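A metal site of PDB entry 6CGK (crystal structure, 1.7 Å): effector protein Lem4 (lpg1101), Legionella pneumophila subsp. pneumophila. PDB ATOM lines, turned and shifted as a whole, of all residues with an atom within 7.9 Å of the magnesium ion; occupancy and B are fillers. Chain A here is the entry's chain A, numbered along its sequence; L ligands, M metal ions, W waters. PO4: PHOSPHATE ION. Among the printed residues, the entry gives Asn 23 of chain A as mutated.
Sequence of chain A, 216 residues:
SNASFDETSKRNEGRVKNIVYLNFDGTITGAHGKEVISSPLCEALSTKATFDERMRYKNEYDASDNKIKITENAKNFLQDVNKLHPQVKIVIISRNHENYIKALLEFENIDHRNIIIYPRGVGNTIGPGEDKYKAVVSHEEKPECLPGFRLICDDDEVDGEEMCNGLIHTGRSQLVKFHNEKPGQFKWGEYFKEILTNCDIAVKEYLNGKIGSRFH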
ATOM      1  N   LEU A  22       8.241  17.011  30.116  1.00  0.00           N
ATOM      2  CA  LEU A  22       9.132  18.059  29.662  1.00  0.00           C
ATOM      3  C   LEU A  22      10.308  18.156  30.618  1.00  0.00           C
ATOM      4  O   LEU A  22      10.110  18.294  31.825  1.00  0.00           O
ATOM      5  CB  LEU A  22       8.416  19.412  29.583  1.00  0.00           C
ATOM      6  CG  LEU A  22       7.082  19.522  28.826  1.00  0.00           C
ATOM      7  CD1 LEU A  22       6.492  20.907  28.940  1.00  0.00           C
ATOM      8  CD2 LEU A  22       7.256  19.131  27.356  1.00  0.00           C
ATOM      9  N   ASN A  23      11.503  18.072  30.070  1.00  0.00           N
ATOM     10  CA  ASN A  23      12.670  18.577  30.755  1.00  0.00           C
ATOM     11  C   ASN A  23      12.513  20.087  30.958  1.00  0.00           C
ATOM     12  O   ASN A  23      11.747  20.747  30.260  1.00  0.00           O
ATOM     13  CB  ASN A  23      13.912  18.267  29.927  1.00  0.00           C
ATOM     14  CG  ASN A  23      15.144  18.731  30.569  1.00  0.00           C
ATOM     15  OD1 ASN A  23      15.819  19.614  30.034  1.00  0.00           O
ATOM     16  ND2 ASN A  23      15.481  18.135  31.705  1.00  0.00           N
ATOM     17  N   PHE A  24      13.248  20.645  31.931  1.00  0.00           N
ATOM     18  CA  PHE A  24      13.133  22.091  32.157  1.00  0.00           C
ATOM     19  C   PHE A  24      14.300  22.874  31.553  1.00  0.00           C
ATOM     20  O   PHE A  24      14.108  23.604  30.578  1.00  0.00           O
ATOM     21  CB  PHE A  24      13.022  22.418  33.645  1.00  0.00           C
ATOM     22  CG  PHE A  24      12.762  23.877  33.927  1.00  0.00           C
ATOM     23  CD1 PHE A  24      11.480  24.402  33.725  1.00  0.00           C
ATOM     24  CD2 PHE A  24      13.762  24.705  34.390  1.00  0.00           C
ATOM     25  CE1 PHE A  24      11.231  25.762  33.985  1.00  0.00           C
ATOM     26  CE2 PHE A  24      13.535  26.064  34.647  1.00  0.00           C
ATOM     27  CZ  PHE A  24      12.253  26.589  34.444  1.00  0.00           C
ATOM     28  N   ASP A  25      15.513  22.733  32.098  1.00  0.00           N
ATOM     29  CA  ASP A  25      16.626  23.571  31.637  1.00  0.00           C
ATOM     30  C   ASP A  25      17.006  23.187  30.216  1.00  0.00           C
ATOM     31  O   ASP A  25      17.324  22.014  29.945  1.00  0.00           O
ATOM     32  CB  ASP A  25      17.856  23.418  32.536  1.00  0.00           C
ATOM     33  CG  ASP A  25      17.603  23.886  33.940  1.00  0.00           C
ATOM     34  OD1 ASP A  25      17.244  25.057  34.112  1.00  0.00           O
ATOM     35  OD2 ASP A  25      17.750  23.071  34.874  1.00  0.00           O
ATOM     36  N   GLY A  26      17.002  24.153  29.327  1.00  0.00           N
ATOM     37  CA  GLY A  26      17.400  23.946  27.952  1.00  0.00           C
ATOM     38  C   GLY A  26      16.278  23.503  27.052  1.00  0.00           C
ATOM     39  O   GLY A  26      16.450  23.488  25.820  1.00  0.00           O
ATOM     40  N   THR A  27      15.157  23.100  27.625  1.00  0.00           N
ATOM     41  CA  THR A  27      13.978  22.679  26.898  1.00  0.00           C
ATOM     42  C   THR A  27      12.892  23.737  27.007  1.00  0.00           C
ATOM     43  O   THR A  27      12.543  24.366  26.007  1.00  0.00           O
ATOM     44  CB  THR A  27      13.487  21.335  27.454  1.00  0.00           C
ATOM     45  OG1 THR A  27      14.534  20.380  27.325  1.00  0.00           O
ATOM     46  CG2 THR A  27      12.286  20.837  26.683  1.00  0.00           C
ATOM     47  N   ILE A  28      12.395  23.979  28.213  1.00  0.00           N
ATOM     48  CA  ILE A  28      11.511  25.109  28.458  1.00  0.00           C
ATOM     49  C   ILE A  28      12.287  26.434  28.495  1.00  0.00           C
ATOM     50  O   ILE A  28      11.765  27.458  28.056  1.00  0.00           O
ATOM     51  CB  ILE A  28      10.718  24.859  29.752  1.00  0.00           C
ATOM     52  CG1 ILE A  28       9.666  23.762  29.482  1.00  0.00           C
ATOM     53  CG2 ILE A  28      10.024  26.136  30.248  1.00  0.00           C
ATOM     54  CD1 ILE A  28       9.176  23.088  30.734  1.00  0.00           C
ATOM     55  N   THR A  29      13.542  26.436  28.976  1.00  0.00           N
ATOM     56  CA  THR A  29      14.378  27.632  28.934  1.00  0.00           C
ATOM     57  C   THR A  29      15.373  27.543  27.789  1.00  0.00           C
ATOM     58  O   THR A  29      15.479  26.528  27.082  1.00  0.00           O
ATOM     59  CB  THR A  29      15.155  27.827  30.243  1.00  0.00           C
ATOM     60  OG1 THR A  29      16.219  26.859  30.310  1.00  0.00           O
ATOM     61  CG2 THR A  29      14.272  27.676  31.448  1.00  0.00           C
ATOM     62  N   ALA A  31      18.715  27.611  28.181  1.00  0.00           N
ATOM     63  CA  ALA A  31      20.041  27.325  28.705  1.00  0.00           C
ATOM     64  C   ALA A  31      20.092  25.923  29.306  1.00  0.00           C
ATOM     65  O   ALA A  31      19.278  25.598  30.177  1.00  0.00           O
ATOM     66  CB  ALA A  31      20.440  28.336  29.763  1.00  0.00           C
ATOM     67  N   HIS A  32      21.052  25.123  28.837  1.00  0.00           N
ATOM     68  CA  HIS A  32      21.290  23.784  29.398  1.00  0.00           C
ATOM     69  C   HIS A  32      21.506  23.873  30.904  1.00  0.00           C
ATOM     70  O   HIS A  32      22.098  24.837  31.412  1.00  0.00           O
ATOM     71  CB  HIS A  32      22.516  23.145  28.710  1.00  0.00           C
ATOM     72  CG  HIS A  32      22.765  21.706  29.091  1.00  0.00           C
ATOM     73  ND1 HIS A  32      23.322  21.345  30.312  1.00  0.00           N
ATOM     74  CD2 HIS A  32      22.580  20.553  28.406  1.00  0.00           C
ATOM     75  CE1 HIS A  32      23.439  20.023  30.357  1.00  0.00           C
ATOM     76  NE2 HIS A  32      23.008  19.521  29.215  1.00  0.00           N
ATOM     77  N   GLY A  33      21.037  22.860  31.619  1.00  0.00           N
ATOM     78  CA  GLY A  33      21.089  22.900  33.066  1.00  0.00           C
ATOM     79  C   GLY A  33      22.495  23.080  33.638  1.00  0.00           C
ATOM     80  O   GLY A  33      22.649  23.669  34.711  1.00  0.00           O
ATOM     81  N   LYS A  34      23.517  22.551  32.949  1.00  0.00           N
ATOM     82  CA  LYS A  34      24.886  22.675  33.463  1.00  0.00           C
ATOM     83  C   LYS A  34      25.274  24.130  33.639  1.00  0.00           C
ATOM     84  O   LYS A  34      26.059  24.460  34.545  1.00  0.00           O
ATOM     85  CB  LYS A  34      25.878  21.971  32.544  1.00  0.00           C
ATOM     86  N   ILE A  93      10.152  17.179  34.477  1.00  0.00           N
ATOM     87  CA  ILE A  93      11.131  16.310  35.132  1.00  0.00           C
ATOM     88  C   ILE A  93      12.494  16.996  34.992  1.00  0.00           C
ATOM     89  O   ILE A  93      12.944  17.243  33.867  1.00  0.00           O
ATOM     90  CB  ILE A  93      11.179  14.889  34.546  1.00  0.00           C
ATOM     91  CG1 ILE A  93       9.784  14.250  34.603  1.00  0.00           C
ATOM     92  CG2 ILE A  93      12.202  14.041  35.323  1.00  0.00           C
ATOM     93  CD1 ILE A  93       9.793  12.765  34.118  1.00  0.00           C
ATOM     94  N   SER A  94      13.121  17.300  36.108  1.00  0.00           N
ATOM     95  CA  SER A  94      14.275  18.192  36.034  1.00  0.00           C
ATOM     96  C   SER A  94      15.235  17.907  37.173  1.00  0.00           C
ATOM     97  O   SER A  94      14.815  17.619  38.297  1.00  0.00           O
ATOM     98  CB  SER A  94      13.827  19.664  36.093  1.00  0.00           C
ATOM     99  OG  SER A  94      14.942  20.550  36.164  1.00  0.00           O
ATOM    100  N   ARG A  95      16.554  18.061  36.900  1.00  0.00           N
ATOM    101  CA  ARG A  95      17.546  18.040  37.968  1.00  0.00           C
ATOM    102  C   ARG A  95      17.697  19.394  38.671  1.00  0.00           C
ATOM    103  O   ARG A  95      18.557  19.510  39.561  1.00  0.00           O
ATOM    104  CB  ARG A  95      18.942  17.653  37.454  1.00  0.00           C
ATOM    105  CG  ARG A  95      19.025  16.469  36.563  1.00  0.00           C
ATOM    106  CD  ARG A  95      20.481  16.104  36.314  1.00  0.00           C
ATOM    107  NE  ARG A  95      20.573  14.918  35.457  1.00  0.00           N
ATOM    108  CZ  ARG A  95      20.580  14.957  34.129  1.00  0.00           C
ATOM    109  NH1 ARG A  95      20.506  16.123  33.489  1.00  0.00           N
ATOM    110  NH2 ARG A  95      20.684  13.820  33.438  1.00  0.00           N
ATOM    111  N   LYS A 132      15.703  10.371  35.711  1.00  0.00           N
ATOM    112  CA  LYS A 132      14.563  10.609  34.814  1.00  0.00           C
ATOM    113  C   LYS A 132      13.872   9.311  34.437  1.00  0.00           C
ATOM    114  O   LYS A 132      12.645   9.268  34.302  1.00  0.00           O
ATOM    115  CB  LYS A 132      15.013  11.307  33.529  1.00  0.00           C
ATOM    116  CG  LYS A 132      15.861  12.563  33.651  1.00  0.00           C
ATOM    117  CD  LYS A 132      15.166  13.655  34.393  1.00  0.00           C
ATOM    118  CE  LYS A 132      16.053  14.922  34.466  1.00  0.00           C
ATOM    119  NZ  LYS A 132      16.376  15.529  33.133  1.00  0.00           N
ATOM    120  N   CYS A 153       9.952  15.911  25.554  1.00  0.00           N
ATOM    121  CA  CYS A 153      10.913  16.879  25.036  1.00  0.00           C
ATOM    122  C   CYS A 153      12.098  16.996  25.996  1.00  0.00           C
ATOM    123  O   CYS A 153      11.911  17.223  27.190  1.00  0.00           O
ATOM    124  CB  CYS A 153      10.263  18.245  24.854  1.00  0.00           C
ATOM    125  SG  CYS A 153       8.956  18.200  23.644  1.00  0.00           S
ATOM    126  N   ASP A 154      13.305  16.830  25.459  1.00  0.00           N
ATOM    127  CA  ASP A 154      14.523  17.006  26.241  1.00  0.00           C
ATOM    128  C   ASP A 154      15.619  17.540  25.328  1.00  0.00           C
ATOM    129  O   ASP A 154      15.710  17.144  24.167  1.00  0.00           O
ATOM    130  CB  ASP A 154      14.954  15.692  26.891  1.00  0.00           C
ATOM    131  CG  ASP A 154      15.772  15.889  28.141  1.00  0.00           C
ATOM    132  OD1 ASP A 154      16.662  16.758  28.155  1.00  0.00           O
ATOM    133  OD2 ASP A 154      15.527  15.159  29.125  1.00  0.00           O
ATOM    134  N   ASP A 155      16.443  18.451  25.860  1.00  0.00           N
ATOM    135  CA  ASP A 155      17.590  18.934  25.099  1.00  0.00           C
ATOM    136  C   ASP A 155      18.822  18.034  25.247  1.00  0.00           C
ATOM    137  O   ASP A 155      19.779  18.185  24.480  1.00  0.00           O
ATOM    138  CB  ASP A 155      17.959  20.344  25.541  1.00  0.00           C
ATOM    139  CG  ASP A 155      18.361  20.398  26.992  1.00  0.00           C
ATOM    140  OD1 ASP A 155      17.553  19.935  27.817  1.00  0.00           O
ATOM    141  OD2 ASP A 155      19.469  20.887  27.317  1.00  0.00           O
ATOM    142  N   ASP A 156      18.829  17.152  26.236  1.00  0.00           N
ATOM    143  CA  ASP A 156      19.906  16.186  26.424  1.00  0.00           C
ATOM    144  C   ASP A 156      19.421  14.860  25.840  1.00  0.00           C
ATOM    145  O   ASP A 156      18.484  14.262  26.362  1.00  0.00           O
ATOM    146  CB  ASP A 156      20.262  16.079  27.915  1.00  0.00           C
ATOM    147  CG  ASP A 156      21.557  15.321  28.155  1.00  0.00           C
ATOM    148  OD1 ASP A 156      21.827  14.350  27.411  1.00  0.00           O
ATOM    149  OD2 ASP A 156      22.305  15.691  29.082  1.00  0.00           O
ATOM    150  N   ASP A 159      19.318  12.024  28.388  1.00  0.00           N
ATOM    151  CA  ASP A 159      18.185  12.235  29.279  1.00  0.00           C
ATOM    152  C   ASP A 159      16.883  11.907  28.588  1.00  0.00           C
ATOM    153  O   ASP A 159      15.993  11.282  29.188  1.00  0.00           O
ATOM    154  CB  ASP A 159      18.129  13.694  29.737  1.00  0.00           C
ATOM    155  CG  ASP A 159      18.937  13.943  30.965  1.00  0.00           C
ATOM    156  OD1 ASP A 159      20.124  13.545  30.972  1.00  0.00           O
ATOM    157  OD2 ASP A 159      18.379  14.533  31.921  1.00  0.00           O
ATOM    158  N   PRO A 183      18.642  23.831  22.723  1.00  0.00           N
ATOM    159  CA  PRO A 183      17.824  24.854  23.377  1.00  0.00           C
ATOM    160  C   PRO A 183      17.489  25.972  22.403  1.00  0.00           C
ATOM    161  O   PRO A 183      18.320  26.392  21.595  1.00  0.00           O
ATOM    162  CB  PRO A 183      18.704  25.344  24.535  1.00  0.00           C
ATOM    163  CG  PRO A 183      19.681  24.230  24.766  1.00  0.00           C
ATOM    164  CD  PRO A 183      19.898  23.557  23.457  1.00  0.00           C
ATOM    165  N   PHE A 186      13.151  24.132  19.753  1.00  0.00           N
ATOM    166  CA  PHE A 186      11.963  23.281  19.839  1.00  0.00           C
ATOM    167  C   PHE A 186      10.784  23.903  19.104  1.00  0.00           C
ATOM    168  O   PHE A 186      10.550  25.112  19.194  1.00  0.00           O
ATOM    169  CB  PHE A 186      11.601  23.039  21.301  1.00  0.00           C
ATOM    170  CG  PHE A 186      12.575  22.167  22.029  1.00  0.00           C
ATOM    171  CD1 PHE A 186      13.725  22.700  22.582  1.00  0.00           C
ATOM    172  CD2 PHE A 186      12.345  20.806  22.155  1.00  0.00           C
ATOM    173  CE1 PHE A 186      14.630  21.885  23.246  1.00  0.00           C
ATOM    174  CE2 PHE A 186      13.240  19.991  22.816  1.00  0.00           C
ATOM    175  CZ  PHE A 186      14.381  20.526  23.366  1.00  0.00           C
HETATM  176  P   PO4 L   1      17.223  19.769  33.672  1.00  0.00           P
HETATM  177  O1  PO4 L   1      15.893  20.494  33.842  1.00  0.00           O
HETATM  178  O2  PO4 L   1      17.186  18.318  34.145  1.00  0.00           O
HETATM  179  O3  PO4 L   1      18.244  20.533  34.498  1.00  0.00           O
HETATM  180  O4  PO4 L   1      17.683  19.853  32.235  1.00  0.00           O
HETATM  181 MG    MG M   1      17.716  20.032  30.076  1.00  0.00          MG
HETATM  182  O   HOH W   1      18.192  18.002  30.107  1.00  0.00           O
HETATM  183  O   HOH W   2      19.701  20.542  30.035  1.00  0.00           O
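The backbone carbonyl oxygen of Ile 93 sits close to the side-chain amide nitrogen of Asn 23. N of Asp 156 sits at hydrogen-bond distance from OD1 of Asp 154 (2.9 Å). The side-chain amide oxygen of Asn 23 sits close to the side-chain hydroxyl of Thr 27 (3.1 Å). N of Asp 155 sits at hydrogen-bond distance from OG1 of Thr 27 (3.1 Å). O of Cys 153 sits at hydrogen-bond distance from N of Asn 23. The side-chain amino group (NZ) of Lys 132 lies close to the side-chain amide nitrogen (ND2) of Asn 23, at 3.1 Å.
Asp 154 touches the magnesium ion (OD1 to MG, 3.9 Å). Of the 23 residues printed, 4 come within 4 Å of the magnesium ion. The nearest printed residue that does not touch the magnesium ion is Thr 27 (4.2 Å).
The magnesium ion is bound by the side-chain amide oxygen of Asn 23 (1.9 Å), the backbone carbonyl oxygen of Asp 25 (2.0 Å), water W2 (2.0 Å), water W1 (2.1 Å), an oxygen (O4) of the ligand (2.2 Å) and the side-chain carboxylate of Asp 155 (2.3 Å).
Water W2 bridges OD2 of Asp 155 (2.7 Å) and N of Gly 33 (3.1 Å). Water W1 lies within hydrogen-bond range of OD1 of Asp 154 (2.8 Å) and ND2 of Asn 23 (3.1 Å).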
